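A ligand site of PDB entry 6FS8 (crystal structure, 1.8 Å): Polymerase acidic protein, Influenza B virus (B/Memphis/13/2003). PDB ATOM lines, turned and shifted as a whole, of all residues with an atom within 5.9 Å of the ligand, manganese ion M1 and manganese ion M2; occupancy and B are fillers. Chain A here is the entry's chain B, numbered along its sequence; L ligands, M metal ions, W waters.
The side-chain carboxylate (OE2) of Glu 128 lies close to the side-chain amino group (NZ) of Lys 143, 2.7 Å away.
The side-chain amino group (NZ) of Lys 143 is in hydrogen-bond range of the side-chain hydroxyl (OH) of Tyr 139, at 3.4 Å.
N of Glu 34 sits at hydrogen-bond distance from O of Met 29 (2.8 Å).
The side-chain sulfur of Met 42 sits close to a fluorine (F2) of the ligand, 3.4 Å away.
Thr 28 touches the ligand.
Phe 32 touches the ligand (CB to F1, 3.0 Å).
Glu 34 touches the ligand.
Asn 45 touches the ligand.
N of Ile 46 touches C12 of the ligand, at 3.8 Å.
NH1 of Arg 93 touches C23 of the ligand (3.3 Å).
OH of Tyr 139 touches C2 of the ligand (3.9 Å).
Of the 21 residues printed, 14 come within 4 Å of the ligand.
Along chain A the residues within 4 Å of the ligand span positions 28 to 143.
The nearest printed residue that does not touch the ligand is Gly 130 (4.3 Å).
Water W5 lies within hydrogen-bond range of OE1 of Glu 128 (2.7 Å) and O of Leu 115 (2.9 Å).
Water W4 lies within hydrogen-bond range of OH of Tyr 139 (2.9 Å) and N of Ile 131 (2.9 Å).
Water W1 lies within hydrogen-bond range of NH1 of Arg 93 (2.8 Å) and O of Leu 115 (3.0 Å).
Manganese ion M2 is bound by an oxygen (O3) of the ligand (2.0 Å), water W5 (2.1 Å), the side-chain carboxylate of Glu 89 (2.1 Å), an oxygen (O2) of the ligand (2.1 Å), water W2 (2.2 Å) and the side-chain carboxylate of Asp 117 (2.2 Å).
NZ of Lys 143 touches manganese ion M1, at 3.99 Å.
Within 4 Å of manganese ion M1: His 49, Asp 117, Glu 128, Val 129 and Lys 143.
The nearest printed residue that does not touch manganese ion M1 is Gly 130 (4.4 Å).
Of the 21 residues printed, 3 come within 4 Å of manganese ion M2.
Along chain A the residues within 4 Å of manganese ion M2 span positions 49 to 117.
The nearest printed residue that does not touch manganese ion M2 is Glu 128 (4.3 Å).
The side-chain carboxylate (OE2) of Glu 128 binds manganese ion M1, at 2.1 Å.
Manganese ion M1 is bound by an oxygen (O1) of the ligand.
OD2 of Asp 117 binds manganese ion M1.
Manganese ion M1 is bound by O of Val 129, at 2.2 Å.
Manganese ion M1 is bound by an oxygen (O2) of the ligand (2.2 Å).
Manganese ion M1 is bound by a ring nitrogen (NE2) of His 49, 2.3 Å away.
Manganese ion M1 has six donor atoms within binding distance.
NZ of Lys 143 sits close to O1 of the ligand.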
ATOM      1  N   THR A  28     -18.368 -18.453  16.759  1.00  0.00           N
ATOM      2  CA  THR A  28     -17.380 -19.525  16.885  1.00  0.00           C
ATOM      3  C   THR A  28     -18.053 -20.906  16.896  1.00  0.00           C
ATOM      4  O   THR A  28     -17.631 -21.821  16.174  1.00  0.00           O
ATOM      5  CB  THR A  28     -16.531 -19.367  18.172  1.00  0.00           C
ATOM      6  OG1 THR A  28     -15.871 -18.086  18.164  1.00  0.00           O
ATOM      7  CG2 THR A  28     -15.456 -20.479  18.261  1.00  0.00           C
ATOM      8  N   MET A  29     -19.098 -21.039  17.695  1.00  0.00           N
ATOM      9  CA  MET A  29     -19.863 -22.280  17.741  1.00  0.00           C
ATOM     10  C   MET A  29     -20.455 -22.632  16.390  1.00  0.00           C
ATOM     11  O   MET A  29     -20.345 -23.794  15.973  1.00  0.00           O
ATOM     12  CB  MET A  29     -20.958 -22.180  18.791  1.00  0.00           C
ATOM     13  CG  MET A  29     -20.372 -22.233  20.185  1.00  0.00           C
ATOM     14  SD  MET A  29     -21.562 -22.218  21.522  1.00  0.00           S
ATOM     15  CE  MET A  29     -22.201 -23.890  21.368  1.00  0.00           C
ATOM     16  N   PHE A  32     -17.983 -24.095  14.009  1.00  0.00           N
ATOM     17  CA  PHE A  32     -17.666 -25.481  14.319  1.00  0.00           C
ATOM     18  C   PHE A  32     -18.916 -26.380  14.270  1.00  0.00           C
ATOM     19  O   PHE A  32     -18.861 -27.518  14.736  1.00  0.00           O
ATOM     20  CB  PHE A  32     -16.984 -25.596  15.715  1.00  0.00           C
ATOM     21  CG  PHE A  32     -15.515 -25.248  15.716  1.00  0.00           C
ATOM     22  CD1 PHE A  32     -15.105 -23.940  15.722  1.00  0.00           C
ATOM     23  CD2 PHE A  32     -14.547 -26.260  15.715  1.00  0.00           C
ATOM     24  CE1 PHE A  32     -13.751 -23.615  15.724  1.00  0.00           C
ATOM     25  CE2 PHE A  32     -13.199 -25.943  15.716  1.00  0.00           C
ATOM     26  CZ  PHE A  32     -12.800 -24.627  15.724  1.00  0.00           C
ATOM     27  N   SER A  33     -20.006 -25.868  13.695  1.00  0.00           N
ATOM     28  CA  SER A  33     -21.297 -26.569  13.595  1.00  0.00           C
ATOM     29  C   SER A  33     -21.865 -27.045  14.923  1.00  0.00           C
ATOM     30  O   SER A  33     -22.398 -28.166  15.016  1.00  0.00           O
ATOM     31  CB  SER A  33     -21.185 -27.736  12.585  1.00  0.00           C
ATOM     32  OG  SER A  33     -20.676 -27.289  11.341  1.00  0.00           O
ATOM     33  N   GLU A  34     -21.744 -26.221  15.959  1.00  0.00           N
ATOM     34  CA  GLU A  34     -22.339 -26.511  17.276  1.00  0.00           C
ATOM     35  C   GLU A  34     -23.447 -25.520  17.544  1.00  0.00           C
ATOM     36  O   GLU A  34     -23.344 -24.346  17.155  1.00  0.00           O
ATOM     37  CB  GLU A  34     -21.291 -26.416  18.383  1.00  0.00           C
ATOM     38  CG  GLU A  34     -20.208 -27.481  18.292  1.00  0.00           C
ATOM     39  CD  GLU A  34     -20.687 -28.866  18.679  1.00  0.00           C
ATOM     40  OE1 GLU A  34     -21.811 -29.017  19.194  1.00  0.00           O
ATOM     41  OE2 GLU A  34     -19.903 -29.823  18.471  1.00  0.00           O
ATOM     42  N   MET A  42     -20.963 -25.454  26.678  1.00  0.00           N
ATOM     43  CA  MET A  42     -19.981 -25.001  25.699  1.00  0.00           C
ATOM     44  C   MET A  42     -20.106 -23.493  25.446  1.00  0.00           C
ATOM     45  O   MET A  42     -19.071 -22.809  25.314  1.00  0.00           O
ATOM     46  CB  MET A  42     -20.099 -25.765  24.371  1.00  0.00           C
ATOM     47  CG  MET A  42     -19.016 -25.399  23.370  1.00  0.00           C
ATOM     48  SD  MET A  42     -19.110 -26.313  21.830  1.00  0.00           S
ATOM     49  CE  MET A  42     -18.895 -27.983  22.431  1.00  0.00           C
ATOM     50  N   ASN A  45     -18.614 -21.685  28.361  1.00  0.00           N
ATOM     51  CA  ASN A  45     -17.153 -21.834  28.373  1.00  0.00           C
ATOM     52  C   ASN A  45     -16.439 -20.965  27.328  1.00  0.00           C
ATOM     53  O   ASN A  45     -15.367 -20.389  27.587  1.00  0.00           O
ATOM     54  CB  ASN A  45     -16.751 -23.301  28.205  1.00  0.00           C
ATOM     55  CG  ASN A  45     -17.090 -24.151  29.414  1.00  0.00           C
ATOM     56  OD1 ASN A  45     -17.096 -23.671  30.563  1.00  0.00           O
ATOM     57  ND2 ASN A  45     -17.384 -25.426  29.157  1.00  0.00           N
ATOM     58  N   ILE A  46     -17.025 -20.884  26.144  1.00  0.00           N
ATOM     59  CA  ILE A  46     -16.473 -20.054  25.073  1.00  0.00           C
ATOM     60  C   ILE A  46     -16.613 -18.581  25.430  1.00  0.00           C
ATOM     61  O   ILE A  46     -15.654 -17.809  25.261  1.00  0.00           O
ATOM     62  CB  ILE A  46     -17.076 -20.420  23.707  1.00  0.00           C
ATOM     63  CG1 ILE A  46     -16.683 -21.852  23.352  1.00  0.00           C
ATOM     64  CG2 ILE A  46     -16.571 -19.485  22.601  1.00  0.00           C
ATOM     65  CD1 ILE A  46     -17.509 -22.421  22.235  1.00  0.00           C
ATOM     66  N   HIS A  49     -14.056 -17.622  28.238  1.00  0.00           N
ATOM     67  CA  HIS A  49     -12.697 -17.653  27.691  1.00  0.00           C
ATOM     68  C   HIS A  49     -12.483 -16.380  26.881  1.00  0.00           C
ATOM     69  O   HIS A  49     -11.443 -15.692  27.048  1.00  0.00           O
ATOM     70  CB  HIS A  49     -12.484 -18.930  26.913  1.00  0.00           C
ATOM     71  CG  HIS A  49     -11.187 -19.034  26.167  1.00  0.00           C
ATOM     72  ND1 HIS A  49     -11.072 -18.638  24.848  1.00  0.00           N
ATOM     73  CD2 HIS A  49     -10.010 -19.637  26.477  1.00  0.00           C
ATOM     74  CE1 HIS A  49      -9.863 -18.928  24.404  1.00  0.00           C
ATOM     75  NE2 HIS A  49      -9.189 -19.509  25.374  1.00  0.00           N
ATOM     76  N   GLU A  89      -8.516 -14.766  19.227  1.00  0.00           N
ATOM     77  CA  GLU A  89      -9.725 -15.555  19.504  1.00  0.00           C
ATOM     78  C   GLU A  89     -10.942 -14.686  19.156  1.00  0.00           C
ATOM     79  O   GLU A  89     -10.841 -13.471  19.100  1.00  0.00           O
ATOM     80  CB  GLU A  89      -9.699 -15.998  20.996  1.00  0.00           C
ATOM     81  CG  GLU A  89     -10.786 -16.958  21.504  1.00  0.00           C
ATOM     82  CD  GLU A  89     -10.788 -18.293  20.771  1.00  0.00           C
ATOM     83  OE1 GLU A  89     -10.069 -19.253  21.165  1.00  0.00           O
ATOM     84  OE2 GLU A  89     -11.480 -18.301  19.738  1.00  0.00           O
ATOM     85  N   ARG A  93     -11.755 -18.381  11.826  1.00  0.00           N
ATOM     86  CA  ARG A  93     -10.366 -18.858  11.765  1.00  0.00           C
ATOM     87  C   ARG A  93      -9.665 -18.469  10.463  1.00  0.00           C
ATOM     88  O   ARG A  93      -8.453 -18.302  10.459  1.00  0.00           O
ATOM     89  CB  ARG A  93     -10.283 -20.361  11.999  1.00  0.00           C
ATOM     90  CG  ARG A  93     -10.657 -20.721  13.426  1.00  0.00           C
ATOM     91  CD  ARG A  93     -10.666 -22.217  13.693  1.00  0.00           C
ATOM     92  NE  ARG A  93      -9.335 -22.843  13.723  1.00  0.00           N
ATOM     93  CZ  ARG A  93      -8.513 -22.896  14.772  1.00  0.00           C
ATOM     94  NH1 ARG A  93      -8.793 -22.277  15.915  1.00  0.00           N
ATOM     95  NH2 ARG A  93      -7.361 -23.537  14.652  1.00  0.00           N
ATOM     96  N   LEU A 115      -3.228 -22.009  16.277  1.00  0.00           N
ATOM     97  CA  LEU A 115      -3.851 -20.690  16.351  1.00  0.00           C
ATOM     98  C   LEU A 115      -3.931 -20.262  17.790  1.00  0.00           C
ATOM     99  O   LEU A 115      -4.559 -20.939  18.618  1.00  0.00           O
ATOM    100  CB  LEU A 115      -5.233 -20.701  15.732  1.00  0.00           C
ATOM    101  CG  LEU A 115      -5.877 -19.326  15.485  1.00  0.00           C
ATOM    102  CD1 LEU A 115      -5.008 -18.462  14.569  1.00  0.00           C
ATOM    103  CD2 LEU A 115      -7.264 -19.530  14.921  1.00  0.00           C
ATOM    104  N   ALA A 116      -3.303 -19.144  18.091  1.00  0.00           N
ATOM    105  CA  ALA A 116      -3.246 -18.629  19.442  1.00  0.00           C
ATOM    106  C   ALA A 116      -4.532 -17.882  19.852  1.00  0.00           C
ATOM    107  O   ALA A 116      -5.453 -17.744  19.074  1.00  0.00           O
ATOM    108  CB  ALA A 116      -2.029 -17.716  19.564  1.00  0.00           C
ATOM    109  N   ASP A 117      -4.552 -17.403  21.095  1.00  0.00           N
ATOM    110  CA  ASP A 117      -5.615 -16.534  21.610  1.00  0.00           C
ATOM    111  C   ASP A 117      -5.308 -15.038  21.586  1.00  0.00           C
ATOM    112  O   ASP A 117      -6.207 -14.223  21.311  1.00  0.00           O
ATOM    113  CB  ASP A 117      -6.005 -16.919  23.035  1.00  0.00           C
ATOM    114  CG  ASP A 117      -6.665 -18.290  23.103  1.00  0.00           C
ATOM    115  OD1 ASP A 117      -7.453 -18.654  22.209  1.00  0.00           O
ATOM    116  OD2 ASP A 117      -6.353 -19.020  24.070  1.00  0.00           O
ATOM    117  N   GLU A 128      -1.556 -18.476  24.556  1.00  0.00           N
ATOM    118  CA  GLU A 128      -2.686 -19.347  24.663  1.00  0.00           C
ATOM    119  C   GLU A 128      -3.278 -19.122  26.035  1.00  0.00           C
ATOM    120  O   GLU A 128      -2.564 -19.245  27.045  1.00  0.00           O
ATOM    121  CB  GLU A 128      -2.255 -20.810  24.502  1.00  0.00           C
ATOM    122  CG  GLU A 128      -3.358 -21.815  24.834  1.00  0.00           C
ATOM    123  CD  GLU A 128      -4.612 -21.671  23.979  1.00  0.00           C
ATOM    124  OE1 GLU A 128      -4.427 -21.297  22.797  1.00  0.00           O
ATOM    125  OE2 GLU A 128      -5.760 -21.979  24.419  1.00  0.00           O
ATOM    126  N   VAL A 129      -4.569 -18.861  26.080  1.00  0.00           N
ATOM    127  CA  VAL A 129      -5.298 -18.656  27.334  1.00  0.00           C
ATOM    128  C   VAL A 129      -6.093 -19.916  27.650  1.00  0.00           C
ATOM    129  O   VAL A 129      -6.736 -20.496  26.787  1.00  0.00           O
ATOM    130  CB  VAL A 129      -6.229 -17.433  27.231  1.00  0.00           C
ATOM    131  CG1 VAL A 129      -7.126 -17.342  28.443  1.00  0.00           C
ATOM    132  CG2 VAL A 129      -5.422 -16.172  27.079  1.00  0.00           C
ATOM    133  N   GLY A 130      -6.047 -20.350  28.907  1.00  0.00           N
ATOM    134  CA  GLY A 130      -6.773 -21.540  29.286  1.00  0.00           C
ATOM    135  C   GLY A 130      -7.550 -21.304  30.532  1.00  0.00           C
ATOM    136  O   GLY A 130      -7.036 -20.647  31.452  1.00  0.00           O
ATOM    137  N   ILE A 131      -8.796 -21.784  30.563  1.00  0.00           N
ATOM    138  CA  ILE A 131      -9.619 -21.693  31.764  1.00  0.00           C
ATOM    139  C   ILE A 131      -9.933 -23.126  32.174  1.00  0.00           C
ATOM    140  O   ILE A 131     -10.267 -23.951  31.318  1.00  0.00           O
ATOM    141  CB  ILE A 131     -10.931 -20.904  31.532  1.00  0.00           C
ATOM    142  CG1 ILE A 131     -10.700 -19.607  30.725  1.00  0.00           C
ATOM    143  CG2 ILE A 131     -11.606 -20.563  32.865  1.00  0.00           C
ATOM    144  CD1 ILE A 131      -9.909 -18.536  31.434  1.00  0.00           C
ATOM    145  N   TYR A 139      -3.638 -28.196  33.951  1.00  0.00           N
ATOM    146  CA  TYR A 139      -4.082 -27.728  32.623  1.00  0.00           C
ATOM    147  C   TYR A 139      -2.911 -27.064  31.912  1.00  0.00           C
ATOM    148  O   TYR A 139      -2.732 -27.244  30.713  1.00  0.00           O
ATOM    149  CB  TYR A 139      -5.256 -26.776  32.754  1.00  0.00           C
ATOM    150  CG  TYR A 139      -5.996 -26.489  31.445  1.00  0.00           C
ATOM    151  CD1 TYR A 139      -6.226 -27.502  30.490  1.00  0.00           C
ATOM    152  CD2 TYR A 139      -6.489 -25.233  31.184  1.00  0.00           C
ATOM    153  CE1 TYR A 139      -6.915 -27.224  29.299  1.00  0.00           C
ATOM    154  CE2 TYR A 139      -7.189 -24.961  30.014  1.00  0.00           C
ATOM    155  CZ  TYR A 139      -7.408 -25.948  29.083  1.00  0.00           C
ATOM    156  OH  TYR A 139      -8.074 -25.639  27.923  1.00  0.00           O
ATOM    157  N   LYS A 143      -1.463 -28.309  28.104  1.00  0.00           N
ATOM    158  CA  LYS A 143      -1.316 -27.403  26.967  1.00  0.00           C
ATOM    159  C   LYS A 143       0.134 -27.336  26.528  1.00  0.00           C
ATOM    160  O   LYS A 143       0.438 -27.240  25.343  1.00  0.00           O
ATOM    161  CB  LYS A 143      -1.811 -26.012  27.315  1.00  0.00           C
ATOM    162  CG  LYS A 143      -3.267 -25.970  27.761  1.00  0.00           C
ATOM    163  CD  LYS A 143      -4.251 -25.865  26.625  1.00  0.00           C
ATOM    164  CE  LYS A 143      -4.888 -24.478  26.586  1.00  0.00           C
ATOM    165  NZ  LYS A 143      -5.987 -24.386  25.604  1.00  0.00           N
ATOM    166  N   LYS A 146       1.399 -30.243  24.294  1.00  0.00           N
ATOM    167  CA  LYS A 146       1.008 -29.936  22.922  1.00  0.00           C
ATOM    168  C   LYS A 146       1.819 -28.765  22.303  1.00  0.00           C
ATOM    169  O   LYS A 146       2.388 -28.906  21.206  1.00  0.00           O
ATOM    170  CB  LYS A 146      -0.498 -29.582  22.931  1.00  0.00           C
ATOM    171  CG  LYS A 146      -1.184 -29.351  21.591  1.00  0.00           C
ATOM    172  CD  LYS A 146      -2.698 -29.140  21.789  1.00  0.00           C
ATOM    173  CE  LYS A 146      -3.413 -28.904  20.466  1.00  0.00           C
ATOM    174  NZ  LYS A 146      -4.890 -29.163  20.348  1.00  0.00           N
HETATM  175  C1  LIG L   1      -9.158 -23.079  24.517  1.00  0.00           C
HETATM  176  N1  LIG L   1     -10.707 -24.344  22.548  1.00  0.00           N
HETATM  177  O1  LIG L   1      -8.472 -22.508  25.427  1.00  0.00           O
HETATM  178  C2  LIG L   1      -9.951 -24.172  24.811  1.00  0.00           C
HETATM  179  O2  LIG L   1      -8.421 -21.549  22.854  1.00  0.00           O
HETATM  180  O3  LIG L   1      -9.220 -21.980  20.333  1.00  0.00           O
HETATM  181  C3  LIG L   1      -9.932 -23.208  22.161  1.00  0.00           C
HETATM  182  O4  LIG L   1      -9.754 -26.245  18.817  1.00  0.00           O
HETATM  183  C4  LIG L   1      -9.128 -22.550  23.112  1.00  0.00           C
HETATM  184  C5  LIG L   1      -9.916 -22.869  20.725  1.00  0.00           C
HETATM  185  C6  LIG L   1     -11.186 -24.967  20.268  1.00  0.00           C
HETATM  186  C7  LIG L   1     -14.559 -25.850  21.184  1.00  0.00           C
HETATM  187  C8  LIG L   1     -14.009 -26.735  22.293  1.00  0.00           C
HETATM  188  C9  LIG L   1     -13.905 -24.409  24.076  1.00  0.00           C
HETATM  189  C10 LIG L   1     -13.254 -23.604  23.112  1.00  0.00           C
HETATM  190  C11 LIG L   1     -14.117 -23.895  25.359  1.00  0.00           C
HETATM  191  C12 LIG L   1     -13.715 -22.614  25.719  1.00  0.00           C
HETATM  192  C13 LIG L   1     -13.068 -21.820  24.782  1.00  0.00           C
HETATM  193  C14 LIG L   1     -12.858 -22.309  23.488  1.00  0.00           C
HETATM  194  C15 LIG L   1     -14.611 -23.783  19.933  1.00  0.00           C
HETATM  195  C16 LIG L   1     -15.667 -24.252  19.180  1.00  0.00           C
HETATM  196  C17 LIG L   1     -16.175 -25.510  19.434  1.00  0.00           C
HETATM  197  C18 LIG L   1     -15.628 -26.308  20.404  1.00  0.00           C
HETATM  198  F1  LIG L   1     -17.199 -26.014  18.704  1.00  0.00           F
HETATM  199  C19 LIG L   1     -14.057 -24.579  20.960  1.00  0.00           C
HETATM  200  F2  LIG L   1     -16.157 -27.525  20.614  1.00  0.00           F
HETATM  201  S1  LIG L   1     -14.500 -26.007  23.836  1.00  0.00           S
HETATM  202  C20 LIG L   1     -12.907 -24.027  21.712  1.00  0.00           C
HETATM  203  N2  LIG L   1     -11.647 -24.920  21.634  1.00  0.00           N
HETATM  204  C21 LIG L   1     -10.219 -26.135  20.170  1.00  0.00           C
HETATM  205  C22 LIG L   1      -9.297 -25.029  18.218  1.00  0.00           C
HETATM  206  C23 LIG L   1     -10.226 -23.837  18.439  1.00  0.00           C
HETATM  207  N3  LIG L   1     -10.443 -23.772  19.861  1.00  0.00           N
HETATM  208  C24 LIG L   1     -10.718 -24.791  23.820  1.00  0.00           C
HETATM  209 MN    MN M   1      -7.428 -20.775  24.716  1.00  0.00          MN
HETATM  210 MN    MN M   2      -8.232 -20.348  21.081  1.00  0.00          MN
HETATM  211  O   HOH W   1      -7.062 -22.550  18.074  1.00  0.00           O
HETATM  212  O   HOH W   2      -7.790 -19.438  19.162  1.00  0.00           O
HETATM  213  O   HOH W   3     -12.279 -21.025  19.704  1.00  0.00           O
HETATM  214  O   HOH W   4      -9.339 -23.049  27.958  1.00  0.00           O
HETATM  215  O   HOH W   5      -6.292 -21.025  20.929  1.00  0.00           O
